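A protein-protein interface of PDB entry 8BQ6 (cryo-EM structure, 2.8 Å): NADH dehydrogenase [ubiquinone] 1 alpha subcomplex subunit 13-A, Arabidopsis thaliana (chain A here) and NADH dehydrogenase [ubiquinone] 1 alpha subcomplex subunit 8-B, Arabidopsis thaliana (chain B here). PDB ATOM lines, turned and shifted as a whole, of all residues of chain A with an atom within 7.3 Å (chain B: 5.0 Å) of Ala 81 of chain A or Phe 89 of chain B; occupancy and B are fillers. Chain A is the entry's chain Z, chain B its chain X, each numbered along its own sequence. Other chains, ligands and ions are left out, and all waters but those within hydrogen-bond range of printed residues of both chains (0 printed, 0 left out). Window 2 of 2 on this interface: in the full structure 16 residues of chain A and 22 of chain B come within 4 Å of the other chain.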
ATOM      1  N   LEU A  74     -11.173 -18.587  26.276  1.00  0.00           N
ATOM      2  CA  LEU A  74      -9.832 -19.127  26.042  1.00  0.00           C
ATOM      3  C   LEU A  74      -9.422 -18.979  24.579  1.00  0.00           C
ATOM      4  O   LEU A  74      -8.308 -18.526  24.257  1.00  0.00           O
ATOM      5  CB  LEU A  74      -9.797 -20.601  26.437  1.00  0.00           C
ATOM      6  CG  LEU A  74      -9.361 -21.035  27.832  1.00  0.00           C
ATOM      7  CD1 LEU A  74      -8.950 -22.489  27.756  1.00  0.00           C
ATOM      8  CD2 LEU A  74      -8.236 -20.173  28.385  1.00  0.00           C
ATOM      9  N   LYS A  75     -10.320 -19.375  23.674  1.00  0.00           N
ATOM     10  CA  LYS A  75     -10.041 -19.240  22.250  1.00  0.00           C
ATOM     11  C   LYS A  75      -9.859 -17.780  21.864  1.00  0.00           C
ATOM     12  O   LYS A  75      -9.036 -17.453  20.999  1.00  0.00           O
ATOM     13  CB  LYS A  75     -11.170 -19.865  21.436  1.00  0.00           C
ATOM     14  CG  LYS A  75     -10.871 -21.252  20.923  1.00  0.00           C
ATOM     15  CD  LYS A  75     -12.155 -21.989  20.609  1.00  0.00           C
ATOM     16  CE  LYS A  75     -12.903 -21.301  19.478  1.00  0.00           C
ATOM     17  NZ  LYS A  75     -12.038 -21.095  18.282  1.00  0.00           N
ATOM     18  N   GLU A  76     -10.632 -16.889  22.484  1.00  0.00           N
ATOM     19  CA  GLU A  76     -10.519 -15.470  22.178  1.00  0.00           C
ATOM     20  C   GLU A  76      -9.170 -14.926  22.622  1.00  0.00           C
ATOM     21  O   GLU A  76      -8.587 -14.077  21.941  1.00  0.00           O
ATOM     22  CB  GLU A  76     -11.660 -14.709  22.854  1.00  0.00           C
ATOM     23  CG  GLU A  76     -12.205 -13.517  22.077  1.00  0.00           C
ATOM     24  CD  GLU A  76     -12.332 -13.792  20.586  1.00  0.00           C
ATOM     25  OE1 GLU A  76     -13.347 -14.391  20.161  1.00  0.00           O
ATOM     26  OE2 GLU A  76     -11.407 -13.418  19.839  1.00  0.00           O
ATOM     27  N   GLU A  77      -8.666 -15.403  23.763  1.00  0.00           N
ATOM     28  CA  GLU A  77      -7.324 -15.038  24.205  1.00  0.00           C
ATOM     29  C   GLU A  77      -6.283 -15.445  23.172  1.00  0.00           C
ATOM     30  O   GLU A  77      -5.421 -14.643  22.780  1.00  0.00           O
ATOM     31  CB  GLU A  77      -7.027 -15.699  25.553  1.00  0.00           C
ATOM     32  CG  GLU A  77      -5.719 -15.275  26.208  1.00  0.00           C
ATOM     33  CD  GLU A  77      -5.266 -16.237  27.298  1.00  0.00           C
ATOM     34  OE1 GLU A  77      -5.955 -17.253  27.528  1.00  0.00           O
ATOM     35  OE2 GLU A  77      -4.232 -15.964  27.945  1.00  0.00           O
ATOM     36  N   LYS A  78      -6.351 -16.696  22.716  1.00  0.00           N
ATOM     37  CA  LYS A  78      -5.355 -17.153  21.749  1.00  0.00           C
ATOM     38  C   LYS A  78      -5.450 -16.371  20.435  1.00  0.00           C
ATOM     39  O   LYS A  78      -4.423 -16.022  19.832  1.00  0.00           O
ATOM     40  CB  LYS A  78      -5.498 -18.655  21.525  1.00  0.00           C
ATOM     41  CG  LYS A  78      -4.527 -19.223  20.524  1.00  0.00           C
ATOM     42  CD  LYS A  78      -4.793 -20.693  20.296  1.00  0.00           C
ATOM     43  CE  LYS A  78      -5.413 -20.926  18.945  1.00  0.00           C
ATOM     44  NZ  LYS A  78      -6.814 -20.463  18.959  1.00  0.00           N
ATOM     45  N   TYR A  79      -6.671 -16.060  19.989  1.00  0.00           N
ATOM     46  CA  TYR A  79      -6.847 -15.286  18.759  1.00  0.00           C
ATOM     47  C   TYR A  79      -6.373 -13.839  18.914  1.00  0.00           C
ATOM     48  O   TYR A  79      -5.861 -13.251  17.954  1.00  0.00           O
ATOM     49  CB  TYR A  79      -8.313 -15.331  18.321  1.00  0.00           C
ATOM     50  CG  TYR A  79      -8.799 -16.695  17.860  1.00  0.00           C
ATOM     51  CD1 TYR A  79      -7.913 -17.676  17.438  1.00  0.00           C
ATOM     52  CD2 TYR A  79     -10.150 -17.007  17.879  1.00  0.00           C
ATOM     53  CE1 TYR A  79      -8.370 -18.918  17.020  1.00  0.00           C
ATOM     54  CE2 TYR A  79     -10.609 -18.245  17.475  1.00  0.00           C
ATOM     55  CZ  TYR A  79      -9.717 -19.197  17.050  1.00  0.00           C
ATOM     56  OH  TYR A  79     -10.187 -20.426  16.648  1.00  0.00           O
ATOM     57  N   ALA A  80      -6.553 -13.240  20.097  1.00  0.00           N
ATOM     58  CA  ALA A  80      -5.965 -11.930  20.363  1.00  0.00           C
ATOM     59  C   ALA A  80      -4.456 -11.982  20.228  1.00  0.00           C
ATOM     60  O   ALA A  80      -3.852 -11.155  19.531  1.00  0.00           O
ATOM     61  CB  ALA A  80      -6.329 -11.456  21.769  1.00  0.00           C
ATOM     62  N   ALA A  81      -3.837 -12.962  20.885  1.00  0.00           N
ATOM     63  CA  ALA A  81      -2.389 -13.080  20.829  1.00  0.00           C
ATOM     64  C   ALA A  81      -1.918 -13.183  19.391  1.00  0.00           C
ATOM     65  O   ALA A  81      -0.963 -12.507  18.990  1.00  0.00           O
ATOM     66  CB  ALA A  81      -1.932 -14.287  21.643  1.00  0.00           C
ATOM     67  N   ARG A  82      -2.614 -13.981  18.581  1.00  0.00           N
ATOM     68  CA  ARG A  82      -2.229 -14.103  17.181  1.00  0.00           C
ATOM     69  C   ARG A  82      -2.426 -12.802  16.411  1.00  0.00           C
ATOM     70  O   ARG A  82      -1.672 -12.521  15.473  1.00  0.00           O
ATOM     71  CB  ARG A  82      -3.016 -15.225  16.525  1.00  0.00           C
ATOM     72  CG  ARG A  82      -2.483 -16.586  16.851  1.00  0.00           C
ATOM     73  CD  ARG A  82      -3.418 -17.633  16.337  1.00  0.00           C
ATOM     74  NE  ARG A  82      -2.988 -18.966  16.725  1.00  0.00           N
ATOM     75  CZ  ARG A  82      -3.406 -20.074  16.135  1.00  0.00           C
ATOM     76  NH1 ARG A  82      -4.264 -20.036  15.128  1.00  0.00           N
ATOM     77  NH2 ARG A  82      -2.942 -21.247  16.553  1.00  0.00           N
ATOM     78  N   ARG A  83      -3.428 -11.999  16.779  1.00  0.00           N
ATOM     79  CA  ARG A  83      -3.701 -10.779  16.023  1.00  0.00           C
ATOM     80  C   ARG A  83      -2.631  -9.717  16.239  1.00  0.00           C
ATOM     81  O   ARG A  83      -2.307  -8.972  15.308  1.00  0.00           O
ATOM     82  CB  ARG A  83      -5.077 -10.224  16.388  1.00  0.00           C
ATOM     83  CG  ARG A  83      -6.199 -10.725  15.495  1.00  0.00           C
ATOM     84  CD  ARG A  83      -7.482  -9.936  15.701  1.00  0.00           C
ATOM     85  NE  ARG A  83      -8.010 -10.146  17.043  1.00  0.00           N
ATOM     86  CZ  ARG A  83      -8.933 -11.045  17.357  1.00  0.00           C
ATOM     87  NH1 ARG A  83      -9.508 -11.796  16.432  1.00  0.00           N
ATOM     88  NH2 ARG A  83      -9.278 -11.202  18.630  1.00  0.00           N
ATOM     89  N   THR A  84      -2.072  -9.624  17.445  1.00  0.00           N
ATOM     90  CA  THR A  84      -1.112  -8.562  17.724  1.00  0.00           C
ATOM     91  C   THR A  84       0.242  -8.809  17.070  1.00  0.00           C
ATOM     92  O   THR A  84       0.883  -7.855  16.619  1.00  0.00           O
ATOM     93  CB  THR A  84      -0.945  -8.383  19.231  1.00  0.00           C
ATOM     94  OG1 THR A  84      -0.152  -9.451  19.757  1.00  0.00           O
ATOM     95  CG2 THR A  84      -2.288  -8.391  19.910  1.00  0.00           C
ATOM     96  N   ILE A  85       0.700 -10.062  17.009  1.00  0.00           N
ATOM     97  CA  ILE A  85       1.970 -10.371  16.362  1.00  0.00           C
ATOM     98  C   ILE A  85       1.816 -10.598  14.874  1.00  0.00           C
ATOM     99  O   ILE A  85       2.803 -10.907  14.195  1.00  0.00           O
ATOM    100  CB  ILE A  85       2.647 -11.595  17.003  1.00  0.00           C
ATOM    101  CG1 ILE A  85       1.790 -12.840  16.787  1.00  0.00           C
ATOM    102  CG2 ILE A  85       2.895 -11.345  18.468  1.00  0.00           C
ATOM    103  CD1 ILE A  85       2.580 -14.107  16.707  1.00  0.00           C
ATOM    104  N   LEU A  86       0.603 -10.475  14.349  1.00  0.00           N
ATOM    105  CA  LEU A  86       0.384 -10.626  12.913  1.00  0.00           C
ATOM    106  C   LEU A  86       1.192  -9.633  12.083  1.00  0.00           C
ATOM    107  O   LEU A  86       1.853 -10.063  11.120  1.00  0.00           O
ATOM    108  CB  LEU A  86      -1.122 -10.516  12.642  1.00  0.00           C
ATOM    109  CG  LEU A  86      -1.703 -10.732  11.249  1.00  0.00           C
ATOM    110  CD1 LEU A  86      -1.700  -9.457  10.432  1.00  0.00           C
ATOM    111  CD2 LEU A  86      -0.913 -11.780  10.568  1.00  0.00           C
ATOM    112  N   THR B  19       4.760 -14.817  20.717  1.00  0.00           N
ATOM    113  CA  THR B  19       3.474 -15.152  21.314  1.00  0.00           C
ATOM    114  C   THR B  19       3.446 -14.797  22.792  1.00  0.00           C
ATOM    115  O   THR B  19       2.447 -14.265  23.289  1.00  0.00           O
ATOM    116  CB  THR B  19       3.171 -16.633  21.117  1.00  0.00           C
ATOM    117  OG1 THR B  19       3.199 -16.939  19.719  1.00  0.00           O
ATOM    118  CG2 THR B  19       1.797 -16.948  21.655  1.00  0.00           C
ATOM    119  N   ALA B  22       3.012 -11.148  23.030  1.00  0.00           N
ATOM    120  CA  ALA B  22       1.944 -10.597  22.201  1.00  0.00           C
ATOM    121  C   ALA B  22       1.096  -9.575  22.945  1.00  0.00           C
ATOM    122  O   ALA B  22       0.663  -8.581  22.356  1.00  0.00           O
ATOM    123  CB  ALA B  22       1.064 -11.728  21.670  1.00  0.00           C
ATOM    124  N   LYS B  23       0.830  -9.800  24.230  1.00  0.00           N
ATOM    125  CA  LYS B  23       0.002  -8.847  24.962  1.00  0.00           C
ATOM    126  C   LYS B  23       0.690  -7.490  25.065  1.00  0.00           C
ATOM    127  O   LYS B  23       0.081  -6.450  24.789  1.00  0.00           O
ATOM    128  CB  LYS B  23      -0.345  -9.402  26.339  1.00  0.00           C
ATOM    129  CG  LYS B  23      -1.691 -10.103  26.366  1.00  0.00           C
ATOM    130  CD  LYS B  23      -1.736 -11.209  27.404  1.00  0.00           C
ATOM    131  CE  LYS B  23      -1.476 -12.565  26.768  1.00  0.00           C
ATOM    132  NZ  LYS B  23      -2.712 -13.219  26.261  1.00  0.00           N
ATOM    133  N   TYR B  78       8.938 -17.813  31.036  1.00  0.00           N
ATOM    134  CA  TYR B  78       7.688 -17.816  30.289  1.00  0.00           C
ATOM    135  C   TYR B  78       7.903 -18.283  28.856  1.00  0.00           C
ATOM    136  O   TYR B  78       7.146 -19.119  28.350  1.00  0.00           O
ATOM    137  CB  TYR B  78       7.062 -16.424  30.313  1.00  0.00           C
ATOM    138  CG  TYR B  78       5.641 -16.400  29.817  1.00  0.00           C
ATOM    139  CD1 TYR B  78       4.853 -17.540  29.863  1.00  0.00           C
ATOM    140  CD2 TYR B  78       5.083 -15.238  29.313  1.00  0.00           C
ATOM    141  CE1 TYR B  78       3.555 -17.524  29.413  1.00  0.00           C
ATOM    142  CE2 TYR B  78       3.783 -15.212  28.863  1.00  0.00           C
ATOM    143  CZ  TYR B  78       3.024 -16.359  28.916  1.00  0.00           C
ATOM    144  OH  TYR B  78       1.725 -16.342  28.469  1.00  0.00           O
ATOM    145  N   MET B  82       6.371 -21.553  27.020  1.00  0.00           N
ATOM    146  CA  MET B  82       5.522 -21.384  25.847  1.00  0.00           C
ATOM    147  C   MET B  82       6.076 -22.155  24.662  1.00  0.00           C
ATOM    148  O   MET B  82       5.315 -22.677  23.838  1.00  0.00           O
ATOM    149  CB  MET B  82       5.390 -19.902  25.512  1.00  0.00           C
ATOM    150  CG  MET B  82       4.305 -19.219  26.312  1.00  0.00           C
ATOM    151  SD  MET B  82       2.639 -19.741  25.884  1.00  0.00           S
ATOM    152  CE  MET B  82       2.282 -18.609  24.557  1.00  0.00           C
ATOM    153  N   ASN B  87       2.953 -22.716  22.665  1.00  0.00           N
ATOM    154  CA  ASN B  87       2.205 -21.463  22.787  1.00  0.00           C
ATOM    155  C   ASN B  87       0.769 -21.670  23.262  1.00  0.00           C
ATOM    156  O   ASN B  87      -0.144 -20.962  22.832  1.00  0.00           O
ATOM    157  CB  ASN B  87       2.217 -20.662  21.479  1.00  0.00           C
ATOM    158  CG  ASN B  87       3.603 -20.539  20.885  1.00  0.00           C
ATOM    159  OD1 ASN B  87       3.760 -20.439  19.671  1.00  0.00           O
ATOM    160  ND2 ASN B  87       4.618 -20.543  21.738  1.00  0.00           N
ATOM    161  N   GLU B  88       0.560 -22.618  24.169  1.00  0.00           N
ATOM    162  CA  GLU B  88      -0.747 -22.828  24.785  1.00  0.00           C
ATOM    163  C   GLU B  88      -0.779 -22.101  26.121  1.00  0.00           C
ATOM    164  O   GLU B  88      -0.071 -22.478  27.061  1.00  0.00           O
ATOM    165  CB  GLU B  88      -1.031 -24.316  24.958  1.00  0.00           C
ATOM    166  CG  GLU B  88      -2.363 -24.739  24.378  1.00  0.00           C
ATOM    167  CD  GLU B  88      -2.412 -24.561  22.875  1.00  0.00           C
ATOM    168  OE1 GLU B  88      -3.434 -24.071  22.355  1.00  0.00           O
ATOM    169  OE2 GLU B  88      -1.413 -24.880  22.212  1.00  0.00           O
ATOM    170  N   PHE B  89      -1.625 -21.073  26.212  1.00  0.00           N
ATOM    171  CA  PHE B  89      -1.578 -20.169  27.356  1.00  0.00           C
ATOM    172  C   PHE B  89      -2.005 -20.858  28.647  1.00  0.00           C
ATOM    173  O   PHE B  89      -1.480 -20.547  29.722  1.00  0.00           O
ATOM    174  CB  PHE B  89      -2.452 -18.947  27.084  1.00  0.00           C
ATOM    175  CG  PHE B  89      -1.867 -18.003  26.080  1.00  0.00           C
ATOM    176  CD1 PHE B  89      -0.829 -17.162  26.431  1.00  0.00           C
ATOM    177  CD2 PHE B  89      -2.353 -17.960  24.786  1.00  0.00           C
ATOM    178  CE1 PHE B  89      -0.287 -16.294  25.510  1.00  0.00           C
ATOM    179  CE2 PHE B  89      -1.813 -17.093  23.861  1.00  0.00           C
ATOM    180  CZ  PHE B  89      -0.779 -16.261  24.225  1.00  0.00           C
ATOM    181  N   ASP B  90      -2.954 -21.794  28.566  1.00  0.00           N
ATOM    182  CA  ASP B  90      -3.517 -22.376  29.782  1.00  0.00           C
ATOM    183  C   ASP B  90      -2.481 -23.167  30.570  1.00  0.00           C
ATOM    184  O   ASP B  90      -2.555 -23.242  31.802  1.00  0.00           O
ATOM    185  CB  ASP B  90      -4.711 -23.265  29.447  1.00  0.00           C
ATOM    186  CG  ASP B  90      -5.864 -23.068  30.410  1.00  0.00           C
ATOM    187  OD1 ASP B  90      -6.958 -23.605  30.147  1.00  0.00           O
ATOM    188  OD2 ASP B  90      -5.674 -22.375  31.433  1.00  0.00           O
ATOM    189  N   LEU B  91      -1.517 -23.770  29.883  1.00  0.00           N
ATOM    190  CA  LEU B  91      -0.481 -24.557  30.540  1.00  0.00           C
ATOM    191  C   LEU B  91       0.662 -23.704  31.072  1.00  0.00           C
ATOM    192  O   LEU B  91       1.608 -24.248  31.653  1.00  0.00           O
ATOM    193  CB  LEU B  91       0.057 -25.616  29.578  1.00  0.00           C
ATOM    194  CG  LEU B  91      -0.984 -26.605  29.052  1.00  0.00           C
ATOM    195  CD1 LEU B  91      -0.530 -27.223  27.745  1.00  0.00           C
ATOM    196  CD2 LEU B  91      -1.242 -27.685  30.083  1.00  0.00           C
ATOM    197  N   CYS B  92       0.590 -22.385  30.894  1.00  0.00           N
ATOM    198  CA  CYS B  92       1.728 -21.507  31.284  1.00  0.00           C
ATOM    199  C   CYS B  92       1.236 -20.371  32.185  1.00  0.00           C
ATOM    200  O   CYS B  92       1.804 -19.273  32.084  1.00  0.00           O
ATOM    201  CB  CYS B  92       2.364 -20.907  30.036  1.00  0.00           C
ATOM    202  SG  CYS B  92       2.738 -22.103  28.727  1.00  0.00           S
ATOM    203  N   ARG B  93       0.245 -20.623  33.049  1.00  0.00           N
ATOM    204  CA  ARG B  93      -0.361 -19.516  33.846  1.00  0.00           C
ATOM    205  C   ARG B  93       0.621 -18.987  34.891  1.00  0.00           C
ATOM    206  O   ARG B  93       0.754 -17.761  34.984  1.00  0.00           O
ATOM    207  CB  ARG B  93      -1.659 -19.975  34.516  1.00  0.00           C
ATOM    208  CG  ARG B  93      -2.778 -20.295  33.537  1.00  0.00           C
ATOM    209  CD  ARG B  93      -3.154 -19.062  32.746  1.00  0.00           C
ATOM    210  NE  ARG B  93      -4.082 -19.385  31.676  1.00  0.00           N
ATOM    211  CZ  ARG B  93      -4.292 -18.627  30.609  1.00  0.00           C
ATOM    212  NH1 ARG B  93      -3.637 -17.490  30.463  1.00  0.00           N
ATOM    213  NH2 ARG B  93      -5.156 -19.014  29.689  1.00  0.00           N
ATOM    214  N   GLN B  96       3.254 -16.883  33.241  1.00  0.00           N
ATOM    215  CA  GLN B  96       2.604 -15.644  32.734  1.00  0.00           C
ATOM    216  C   GLN B  96       2.397 -14.673  33.900  1.00  0.00           C
ATOM    217  O   GLN B  96       2.776 -13.510  33.754  1.00  0.00           O
ATOM    218  CB  GLN B  96       1.255 -15.974  32.099  1.00  0.00           C
ATOM    219  CG  GLN B  96       0.612 -14.806  31.371  1.00  0.00           C
ATOM    220  CD  GLN B  96      -0.738 -15.168  30.806  1.00  0.00           C
ATOM    221  OE1 GLN B  96      -0.895 -16.164  30.105  1.00  0.00           O
ATOM    222  NE2 GLN B  96      -1.733 -14.351  31.110  1.00  0.00           N
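NZ of Lys 23 of chain B lies within salt-bridge range of OE2 of Glu 77 of chain A. The guanidinium group (NH2) of Arg 93 of chain B is in salt-bridge range of the side-chain carboxylate (OE1) of Glu 77 of chain A (2.9 Å). O of Ala 22 of chain B is in hydrogen-bond range of OG1 of Thr 84 of chain A (2.9 Å).
The backbone carbonyl oxygen of Ala 81 of chain A sits at hydrogen-bond distance from the side-chain hydroxyl of Thr 84 of chain A (3.3 Å). The guanidinium group (NH1) of Arg 93 of chain B sits at hydrogen-bond distance from the side-chain amide oxygen (OE1) of Gln 96 of chain B. The backbone carbonyl oxygen of Phe 89 of chain B lies within hydrogen-bond range of the guanidinium group of Arg 93 of chain B, 3.5 Å away. The guanidinium group of Arg 93 of chain B is in salt-bridge range of the side-chain carboxylate of Asp 90 of chain B (3.4 Å). The side-chain hydroxyl (OH) of Tyr 78 of chain B is in hydrogen-bond range of the side-chain amide oxygen (OE1) of Gln 96 of chain B, at 3.1 Å.
Among the printed residues, pairs that only touch across the chains: Leu 74 of chain A with Asp 90 of chain B, Leu 74 of chain A with Arg 93 of chain B, Glu 77 of chain A with Phe 89 of chain B, Glu 77 of chain A with Gln 96 of chain B, Ala 81 of chain A with Ala 22 of chain B, Ala 81 of chain A with Phe 89 of chain B and Ile 85 of chain A with Ala 22 of chain B.
Of the printed residues of chain B, Ala 81 of chain A touches Ala 22 and Phe 89. Of chain A, only Glu 77 and Ala 81 come within 4 Å of Phe 89 of chain B. Of the printed residues of chain A, Ala 22 of chain B touches Ala 81 (3.4 Å), Thr 84 (2.9 Å) and Ile 85 (3.7 Å). Of the printed residues of chain B, Leu 74 of chain A touches Asp 90 and Arg 93. Printed residues of chain A within 4 Å of Gln 96 of chain B: Glu 77 (3.98 Å). Printed residues of chain A within 4 Å of Asp 90 of chain B: Leu 74 (3.3 Å). Of the printed residues of chain B, Thr 84 of chain A touches Ala 22 (2.9 Å).
Of the 13 printed residues of chain A, 5 touch a printed residue of chain B. Of the 13 printed residues of chain B, 6 touch a printed residue of chain A.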
